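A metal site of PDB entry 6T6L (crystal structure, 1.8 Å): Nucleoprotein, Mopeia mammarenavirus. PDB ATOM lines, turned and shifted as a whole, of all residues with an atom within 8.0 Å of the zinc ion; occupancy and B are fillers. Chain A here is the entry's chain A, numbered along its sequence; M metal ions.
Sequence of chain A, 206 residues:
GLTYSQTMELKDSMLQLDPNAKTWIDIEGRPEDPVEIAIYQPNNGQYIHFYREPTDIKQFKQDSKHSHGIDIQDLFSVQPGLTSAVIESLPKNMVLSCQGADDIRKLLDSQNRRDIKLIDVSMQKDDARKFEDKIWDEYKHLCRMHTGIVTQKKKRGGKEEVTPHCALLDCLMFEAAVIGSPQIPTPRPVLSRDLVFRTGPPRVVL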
ATOM      1  N   GLU A  28       2.925   1.458 -19.402  1.00  0.00           N
ATOM      2  CA  GLU A  28       3.935   1.001 -20.347  1.00  0.00           C
ATOM      3  C   GLU A  28       3.410  -0.249 -21.023  1.00  0.00           C
ATOM      4  O   GLU A  28       2.687  -1.034 -20.405  1.00  0.00           O
ATOM      5  CB  GLU A  28       5.287   0.707 -19.652  1.00  0.00           C
ATOM      6  CG  GLU A  28       5.864   1.907 -18.865  1.00  0.00           C
ATOM      7  CD  GLU A  28       6.069   3.151 -19.715  1.00  0.00           C
ATOM      8  OE1 GLU A  28       6.415   3.019 -20.921  1.00  0.00           O
ATOM      9  OE2 GLU A  28       5.911   4.278 -19.169  1.00  0.00           O
ATOM     10  N   VAL A  35       1.897  -3.734 -19.569  1.00  0.00           N
ATOM     11  CA  VAL A  35       2.751  -4.448 -18.613  1.00  0.00           C
ATOM     12  C   VAL A  35       3.016  -3.664 -17.343  1.00  0.00           C
ATOM     13  O   VAL A  35       3.497  -4.248 -16.358  1.00  0.00           O
ATOM     14  CB  VAL A  35       4.105  -4.861 -19.240  1.00  0.00           C
ATOM     15  CG1 VAL A  35       3.869  -5.815 -20.411  1.00  0.00           C
ATOM     16  CG2 VAL A  35       4.913  -3.624 -19.664  1.00  0.00           C
ATOM     17  N   GLU A  36       2.752  -2.362 -17.299  1.00  0.00           N
ATOM     18  CA  GLU A  36       2.976  -1.599 -16.080  1.00  0.00           C
ATOM     19  C   GLU A  36       1.969  -0.472 -16.085  1.00  0.00           C
ATOM     20  O   GLU A  36       1.804   0.219 -17.100  1.00  0.00           O
ATOM     21  CB  GLU A  36       4.413  -1.060 -15.980  1.00  0.00           C
ATOM     22  CG  GLU A  36       4.703  -0.402 -14.637  1.00  0.00           C
ATOM     23  CD  GLU A  36       6.097   0.224 -14.585  1.00  0.00           C
ATOM     24  OE1 GLU A  36       6.593   0.676 -15.631  1.00  0.00           O
ATOM     25  OE2 GLU A  36       6.668   0.251 -13.472  1.00  0.00           O
ATOM     26  N   ILE A  37       1.287  -0.289 -14.962  1.00  0.00           N
ATOM     27  CA  ILE A  37       0.272   0.751 -14.830  1.00  0.00           C
ATOM     28  C   ILE A  37       0.519   1.510 -13.532  1.00  0.00           C
ATOM     29  O   ILE A  37       0.793   0.913 -12.489  1.00  0.00           O
ATOM     30  CB  ILE A  37      -1.146   0.152 -14.863  1.00  0.00           C
ATOM     31  CG1 ILE A  37      -1.473  -0.398 -16.254  1.00  0.00           C
ATOM     32  CG2 ILE A  37      -2.184   1.206 -14.518  1.00  0.00           C
ATOM     33  CD1 ILE A  37      -2.236  -1.703 -16.237  1.00  0.00           C
ATOM     34  N   ALA A  38       0.415   2.844 -13.596  1.00  0.00           N
ATOM     35  CA  ALA A  38       0.511   3.672 -12.400  1.00  0.00           C
ATOM     36  C   ALA A  38      -0.594   4.721 -12.410  1.00  0.00           C
ATOM     37  O   ALA A  38      -0.896   5.326 -13.450  1.00  0.00           O
ATOM     38  CB  ALA A  38       1.879   4.359 -12.284  1.00  0.00           C
ATOM     39  N   HIS A  49       0.091   1.104  -8.267  1.00  0.00           N
ATOM     40  CA  HIS A  49       1.159   0.780  -9.206  1.00  0.00           C
ATOM     41  C   HIS A  49       1.341  -0.739  -9.223  1.00  0.00           C
ATOM     42  O   HIS A  49       1.446  -1.355  -8.165  1.00  0.00           O
ATOM     43  CB  HIS A  49       2.467   1.488  -8.803  1.00  0.00           C
ATOM     44  CG  HIS A  49       3.653   1.109  -9.630  1.00  0.00           C
ATOM     45  ND1 HIS A  49       4.902   0.891  -9.088  1.00  0.00           N
ATOM     46  CD2 HIS A  49       3.796   0.948 -10.970  1.00  0.00           C
ATOM     47  CE1 HIS A  49       5.759   0.587 -10.046  1.00  0.00           C
ATOM     48  NE2 HIS A  49       5.114   0.604 -11.201  1.00  0.00           N
ATOM     49  N   PHE A  50       1.334  -1.327 -10.417  1.00  0.00           N
ATOM     50  CA  PHE A  50       1.421  -2.783 -10.524  1.00  0.00           C
ATOM     51  C   PHE A  50       1.868  -3.138 -11.941  1.00  0.00           C
ATOM     52  O   PHE A  50       2.001  -2.270 -12.807  1.00  0.00           O
ATOM     53  CB  PHE A  50       0.079  -3.450 -10.173  1.00  0.00           C
ATOM     54  CG  PHE A  50      -1.048  -2.978 -11.021  1.00  0.00           C
ATOM     55  CD1 PHE A  50      -1.381  -3.665 -12.185  1.00  0.00           C
ATOM     56  CD2 PHE A  50      -1.770  -1.831 -10.679  1.00  0.00           C
ATOM     57  CE1 PHE A  50      -2.419  -3.215 -13.000  1.00  0.00           C
ATOM     58  CE2 PHE A  50      -2.821  -1.387 -11.497  1.00  0.00           C
ATOM     59  CZ  PHE A  50      -3.135  -2.070 -12.652  1.00  0.00           C
ATOM     60  N   TYR A  51       2.063  -4.439 -12.167  1.00  0.00           N
ATOM     61  CA  TYR A  51       2.641  -4.967 -13.399  1.00  0.00           C
ATOM     62  C   TYR A  51       1.736  -6.046 -13.968  1.00  0.00           C
ATOM     63  O   TYR A  51       0.799  -6.507 -13.335  1.00  0.00           O
ATOM     64  CB  TYR A  51       4.026  -5.555 -13.136  1.00  0.00           C
ATOM     65  CG  TYR A  51       4.910  -4.681 -12.286  1.00  0.00           C
ATOM     66  CD1 TYR A  51       5.665  -3.666 -12.871  1.00  0.00           C
ATOM     67  CD2 TYR A  51       4.989  -4.869 -10.917  1.00  0.00           C
ATOM     68  CE1 TYR A  51       6.492  -2.848 -12.111  1.00  0.00           C
ATOM     69  CE2 TYR A  51       5.824  -4.077 -10.144  1.00  0.00           C
ATOM     70  CZ  TYR A  51       6.571  -3.073 -10.738  1.00  0.00           C
ATOM     71  OH  TYR A  51       7.370  -2.284  -9.970  1.00  0.00           O
ATOM     72  N   HIS A  68      10.696   0.542 -22.029  1.00  0.00           N
ATOM     73  CA  HIS A  68      10.661   0.338 -20.583  1.00  0.00           C
ATOM     74  C   HIS A  68      11.788  -0.500 -20.015  1.00  0.00           C
ATOM     75  O   HIS A  68      11.992  -0.446 -18.803  1.00  0.00           O
ATOM     76  CB  HIS A  68       9.321  -0.265 -20.124  1.00  0.00           C
ATOM     77  CG  HIS A  68       8.906  -1.494 -20.871  1.00  0.00           C
ATOM     78  ND1 HIS A  68       9.586  -2.695 -20.784  1.00  0.00           N
ATOM     79  CD2 HIS A  68       7.845  -1.731 -21.684  1.00  0.00           C
ATOM     80  CE1 HIS A  68       8.970  -3.607 -21.516  1.00  0.00           C
ATOM     81  NE2 HIS A  68       7.914  -3.037 -22.077  1.00  0.00           N
ATOM     82  N   ILE A  70      12.177  -3.560 -19.259  1.00  0.00           N
ATOM     83  CA  ILE A  70      11.808  -4.608 -18.320  1.00  0.00           C
ATOM     84  C   ILE A  70      12.188  -5.960 -18.906  1.00  0.00           C
ATOM     85  O   ILE A  70      11.926  -6.234 -20.087  1.00  0.00           O
ATOM     86  CB  ILE A  70      10.294  -4.558 -18.004  1.00  0.00           C
ATOM     87  CG1 ILE A  70       9.908  -3.240 -17.361  1.00  0.00           C
ATOM     88  CG2 ILE A  70       9.882  -5.739 -17.104  1.00  0.00           C
ATOM     89  CD1 ILE A  70       8.400  -3.067 -17.245  1.00  0.00           C
ATOM     90  N   TRP A 136      14.461  10.227 -10.815  1.00  0.00           N
ATOM     91  CA  TRP A 136      15.125   8.940 -10.629  1.00  0.00           C
ATOM     92  C   TRP A 136      16.060   8.979  -9.428  1.00  0.00           C
ATOM     93  O   TRP A 136      16.116   8.024  -8.661  1.00  0.00           O
ATOM     94  CB  TRP A 136      15.864   8.531 -11.898  1.00  0.00           C
ATOM     95  CG  TRP A 136      14.964   7.871 -12.896  1.00  0.00           C
ATOM     96  CD1 TRP A 136      14.252   8.482 -13.890  1.00  0.00           C
ATOM     97  CD2 TRP A 136      14.638   6.477 -12.980  1.00  0.00           C
ATOM     98  NE1 TRP A 136      13.523   7.557 -14.592  1.00  0.00           N
ATOM     99  CE2 TRP A 136      13.746   6.313 -14.053  1.00  0.00           C
ATOM    100  CE3 TRP A 136      15.024   5.354 -12.251  1.00  0.00           C
ATOM    101  CZ2 TRP A 136      13.225   5.075 -14.423  1.00  0.00           C
ATOM    102  CZ3 TRP A 136      14.510   4.114 -12.615  1.00  0.00           C
ATOM    103  CH2 TRP A 136      13.618   3.987 -13.691  1.00  0.00           C
ATOM    104  N   LYS A 140      14.148   6.277  -7.401  1.00  0.00           N
ATOM    105  CA  LYS A 140      14.502   5.037  -8.093  1.00  0.00           C
ATOM    106  C   LYS A 140      14.124   3.806  -7.276  1.00  0.00           C
ATOM    107  O   LYS A 140      13.846   2.747  -7.849  1.00  0.00           O
ATOM    108  CB  LYS A 140      16.001   5.002  -8.371  1.00  0.00           C
ATOM    109  CG  LYS A 140      16.867   5.016  -7.102  1.00  0.00           C
ATOM    110  CD  LYS A 140      18.366   5.191  -7.378  1.00  0.00           C
ATOM    111  CE  LYS A 140      18.778   6.670  -7.348  1.00  0.00           C
ATOM    112  NZ  LYS A 140      19.433   7.074  -6.062  1.00  0.00           N
ATOM    113  N   LEU A 142      11.508   3.139  -5.761  1.00  0.00           N
ATOM    114  CA  LEU A 142      10.094   2.794  -5.829  1.00  0.00           C
ATOM    115  C   LEU A 142       9.788   1.775  -6.910  1.00  0.00           C
ATOM    116  O   LEU A 142       8.733   1.128  -6.844  1.00  0.00           O
ATOM    117  CB  LEU A 142       9.242   4.047  -6.030  1.00  0.00           C
ATOM    118  CG  LEU A 142       9.289   5.015  -4.859  1.00  0.00           C
ATOM    119  CD1 LEU A 142       8.403   6.231  -5.078  1.00  0.00           C
ATOM    120  CD2 LEU A 142       8.935   4.294  -3.564  1.00  0.00           C
ATOM    121  N   CYS A 143      10.688   1.570  -7.871  1.00  0.00           N
ATOM    122  CA  CYS A 143      10.469   0.551  -8.880  1.00  0.00           C
ATOM    123  C   CYS A 143      11.809   0.093  -9.429  1.00  0.00           C
ATOM    124  O   CYS A 143      12.554   0.872 -10.028  1.00  0.00           O
ATOM    125  CB  CYS A 143       9.592   1.051 -10.044  1.00  0.00           C
ATOM    126  SG  CYS A 143       9.204  -0.195 -11.285  1.00  0.00           S
ATOM    127  N   ARG A 144      12.061  -1.204  -9.260  1.00  0.00           N
ATOM    128  CA  ARG A 144      13.273  -1.908  -9.633  1.00  0.00           C
ATOM    129  C   ARG A 144      13.216  -2.704 -10.925  1.00  0.00           C
ATOM    130  O   ARG A 144      14.159  -3.462 -11.228  1.00  0.00           O
ATOM    131  CB  ARG A 144      13.675  -2.842  -8.482  1.00  0.00           C
ATOM    132  N   MET A 145      12.140  -2.544 -11.693  1.00  0.00           N
ATOM    133  CA  MET A 145      11.866  -3.442 -12.804  1.00  0.00           C
ATOM    134  C   MET A 145      12.597  -3.071 -14.090  1.00  0.00           C
ATOM    135  O   MET A 145      12.597  -3.850 -15.044  1.00  0.00           O
ATOM    136  CB  MET A 145      10.342  -3.461 -13.034  1.00  0.00           C
ATOM    137  CG  MET A 145       9.786  -4.620 -13.785  1.00  0.00           C
ATOM    138  SD  MET A 145       9.616  -6.171 -12.870  1.00  0.00           S
ATOM    139  CE  MET A 145       9.820  -5.715 -11.170  1.00  0.00           C
ATOM    140  N   HIS A 146      13.212  -1.892 -14.148  1.00  0.00           N
ATOM    141  CA  HIS A 146      13.715  -1.378 -15.412  1.00  0.00           C
ATOM    142  C   HIS A 146      15.233  -1.599 -15.477  1.00  0.00           C
ATOM    143  O   HIS A 146      16.042  -0.715 -15.212  1.00  0.00           O
ATOM    144  CB  HIS A 146      13.305   0.087 -15.568  1.00  0.00           C
ATOM    145  CG  HIS A 146      11.829   0.294 -15.417  1.00  0.00           C
ATOM    146  ND1 HIS A 146      10.949   0.145 -16.467  1.00  0.00           N
ATOM    147  CD2 HIS A 146      11.077   0.562 -14.328  1.00  0.00           C
ATOM    148  CE1 HIS A 146       9.707   0.324 -16.034  1.00  0.00           C
ATOM    149  NE2 HIS A 146       9.756   0.553 -14.736  1.00  0.00           N
ATOM    150  N   PRO A 164      15.255   4.359 -19.048  1.00  0.00           N
ATOM    151  CA  PRO A 164      14.030   3.581 -19.258  1.00  0.00           C
ATOM    152  C   PRO A 164      12.808   4.320 -18.742  1.00  0.00           C
ATOM    153  O   PRO A 164      12.891   5.144 -17.822  1.00  0.00           O
ATOM    154  CB  PRO A 164      14.287   2.296 -18.479  1.00  0.00           C
ATOM    155  CG  PRO A 164      15.794   2.159 -18.492  1.00  0.00           C
ATOM    156  CD  PRO A 164      16.310   3.577 -18.382  1.00  0.00           C
ATOM    157  N   HIS A 165      11.659   4.040 -19.362  1.00  0.00           N
ATOM    158  CA  HIS A 165      10.393   4.631 -18.948  1.00  0.00           C
ATOM    159  C   HIS A 165       9.683   3.713 -17.956  1.00  0.00           C
ATOM    160  O   HIS A 165       9.373   2.554 -18.263  1.00  0.00           O
ATOM    161  CB  HIS A 165       9.530   4.892 -20.183  1.00  0.00           C
ATOM    162  CG  HIS A 165      10.092   5.930 -21.110  1.00  0.00           C
ATOM    163  ND1 HIS A 165       9.499   6.257 -22.307  1.00  0.00           N
ATOM    164  CD2 HIS A 165      11.190   6.724 -20.998  1.00  0.00           C
ATOM    165  CE1 HIS A 165      10.203   7.212 -22.899  1.00  0.00           C
ATOM    166  NE2 HIS A 165      11.238   7.512 -22.130  1.00  0.00           N
ATOM    167  N   CYS A 166       9.368   4.260 -16.797  1.00  0.00           N
ATOM    168  CA  CYS A 166       8.591   3.591 -15.763  1.00  0.00           C
ATOM    169  C   CYS A 166       7.270   4.340 -15.591  1.00  0.00           C
ATOM    170  O   CYS A 166       7.265   5.580 -15.519  1.00  0.00           O
ATOM    171  CB  CYS A 166       9.403   3.614 -14.446  1.00  0.00           C
ATOM    172  SG  CYS A 166       8.440   3.290 -12.901  1.00  0.00           S
ATOM    173  N   ALA A 167       6.169   3.603 -15.562  1.00  0.00           N
ATOM    174  CA  ALA A 167       4.872   4.276 -15.516  1.00  0.00           C
ATOM    175  C   ALA A 167       4.753   5.127 -14.254  1.00  0.00           C
ATOM    176  O   ALA A 167       4.185   6.217 -14.302  1.00  0.00           O
ATOM    177  CB  ALA A 167       3.733   3.262 -15.603  1.00  0.00           C
ATOM    178  N   LEU A 168       5.323   4.646 -13.140  1.00  0.00           N
ATOM    179  CA  LEU A 168       5.215   5.391 -11.893  1.00  0.00           C
ATOM    180  C   LEU A 168       6.105   6.630 -11.919  1.00  0.00           C
ATOM    181  O   LEU A 168       5.643   7.731 -11.622  1.00  0.00           O
ATOM    182  CB  LEU A 168       5.585   4.510 -10.705  1.00  0.00           C
ATOM    183  CG  LEU A 168       5.687   5.233  -9.363  1.00  0.00           C
ATOM    184  CD1 LEU A 168       4.362   5.901  -8.983  1.00  0.00           C
ATOM    185  CD2 LEU A 168       6.166   4.250  -8.282  1.00  0.00           C
ATOM    186  N   LEU A 169       7.375   6.464 -12.256  1.00  0.00           N
ATOM    187  CA  LEU A 169       8.256   7.628 -12.203  1.00  0.00           C
ATOM    188  C   LEU A 169       7.900   8.625 -13.294  1.00  0.00           C
ATOM    189  O   LEU A 169       8.106   9.834 -13.115  1.00  0.00           O
ATOM    190  CB  LEU A 169       9.716   7.176 -12.288  1.00  0.00           C
ATOM    191  CG  LEU A 169      10.384   6.954 -10.898  1.00  0.00           C
ATOM    192  CD1 LEU A 169       9.578   6.048  -9.995  1.00  0.00           C
ATOM    193  CD2 LEU A 169      11.814   6.411 -11.054  1.00  0.00           C
ATOM    194  N   ASP A 170       7.317   8.163 -14.403  1.00  0.00           N
ATOM    195  CA  ASP A 170       6.790   9.087 -15.402  1.00  0.00           C
ATOM    196  C   ASP A 170       5.702   9.981 -14.805  1.00  0.00           C
ATOM    197  O   ASP A 170       5.727  11.205 -14.970  1.00  0.00           O
ATOM    198  CB  ASP A 170       6.263   8.334 -16.630  1.00  0.00           C
ATOM    199  CG  ASP A 170       7.368   7.878 -17.573  1.00  0.00           C
ATOM    200  OD1 ASP A 170       8.541   8.197 -17.305  1.00  0.00           O
ATOM    201  OD2 ASP A 170       7.080   7.206 -18.585  1.00  0.00           O
HETATM  202 ZN    ZN M   1       8.462   1.001 -13.124  1.00  0.00          ZN
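OE2 of Glu 36 binds the zinc ion (2.0 Å).
The zinc ion is bound by NE2 of His 146.
The side-chain sulfur (SG) of Cys 166 binds the zinc ion (2.3 Å).
SG of Cys 143 binds the zinc ion (2.3 Å).
The zinc ion has four donor atoms within binding distance.
A ring nitrogen (NE2) of His 49 lies close to the side-chain carboxylate (OE2) of Glu 36 (2.8 Å).
The backbone NH (N) of Ala 167 is in hydrogen-bond range of the side-chain carboxylate (OE1) of Glu 36 (3.0 Å).
N of Glu 28 is in hydrogen-bond range of O of Glu 36 (2.8 Å).
A ring nitrogen (ND1) of His 146 sits at hydrogen-bond distance from the backbone carbonyl oxygen (O) of His 68, 2.6 Å away.
SG of Cys 166 sits close to N of Leu 168 (3.4 Å).
The backbone NH of Leu 169 sits close to the side-chain sulfur of Cys 166 (3.4 Å).
OH of Tyr 51 sits close to SG of Cys 143 (3.1 Å).
SG of Cys 143 sits close to N of Met 145.
Residues that only touch the zinc ion: His 49.
Of the 24 residues printed, 5 come within 4 Å of the zinc ion.
Along chain A the residues within 4 Å of the zinc ion span positions 36 to 166.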
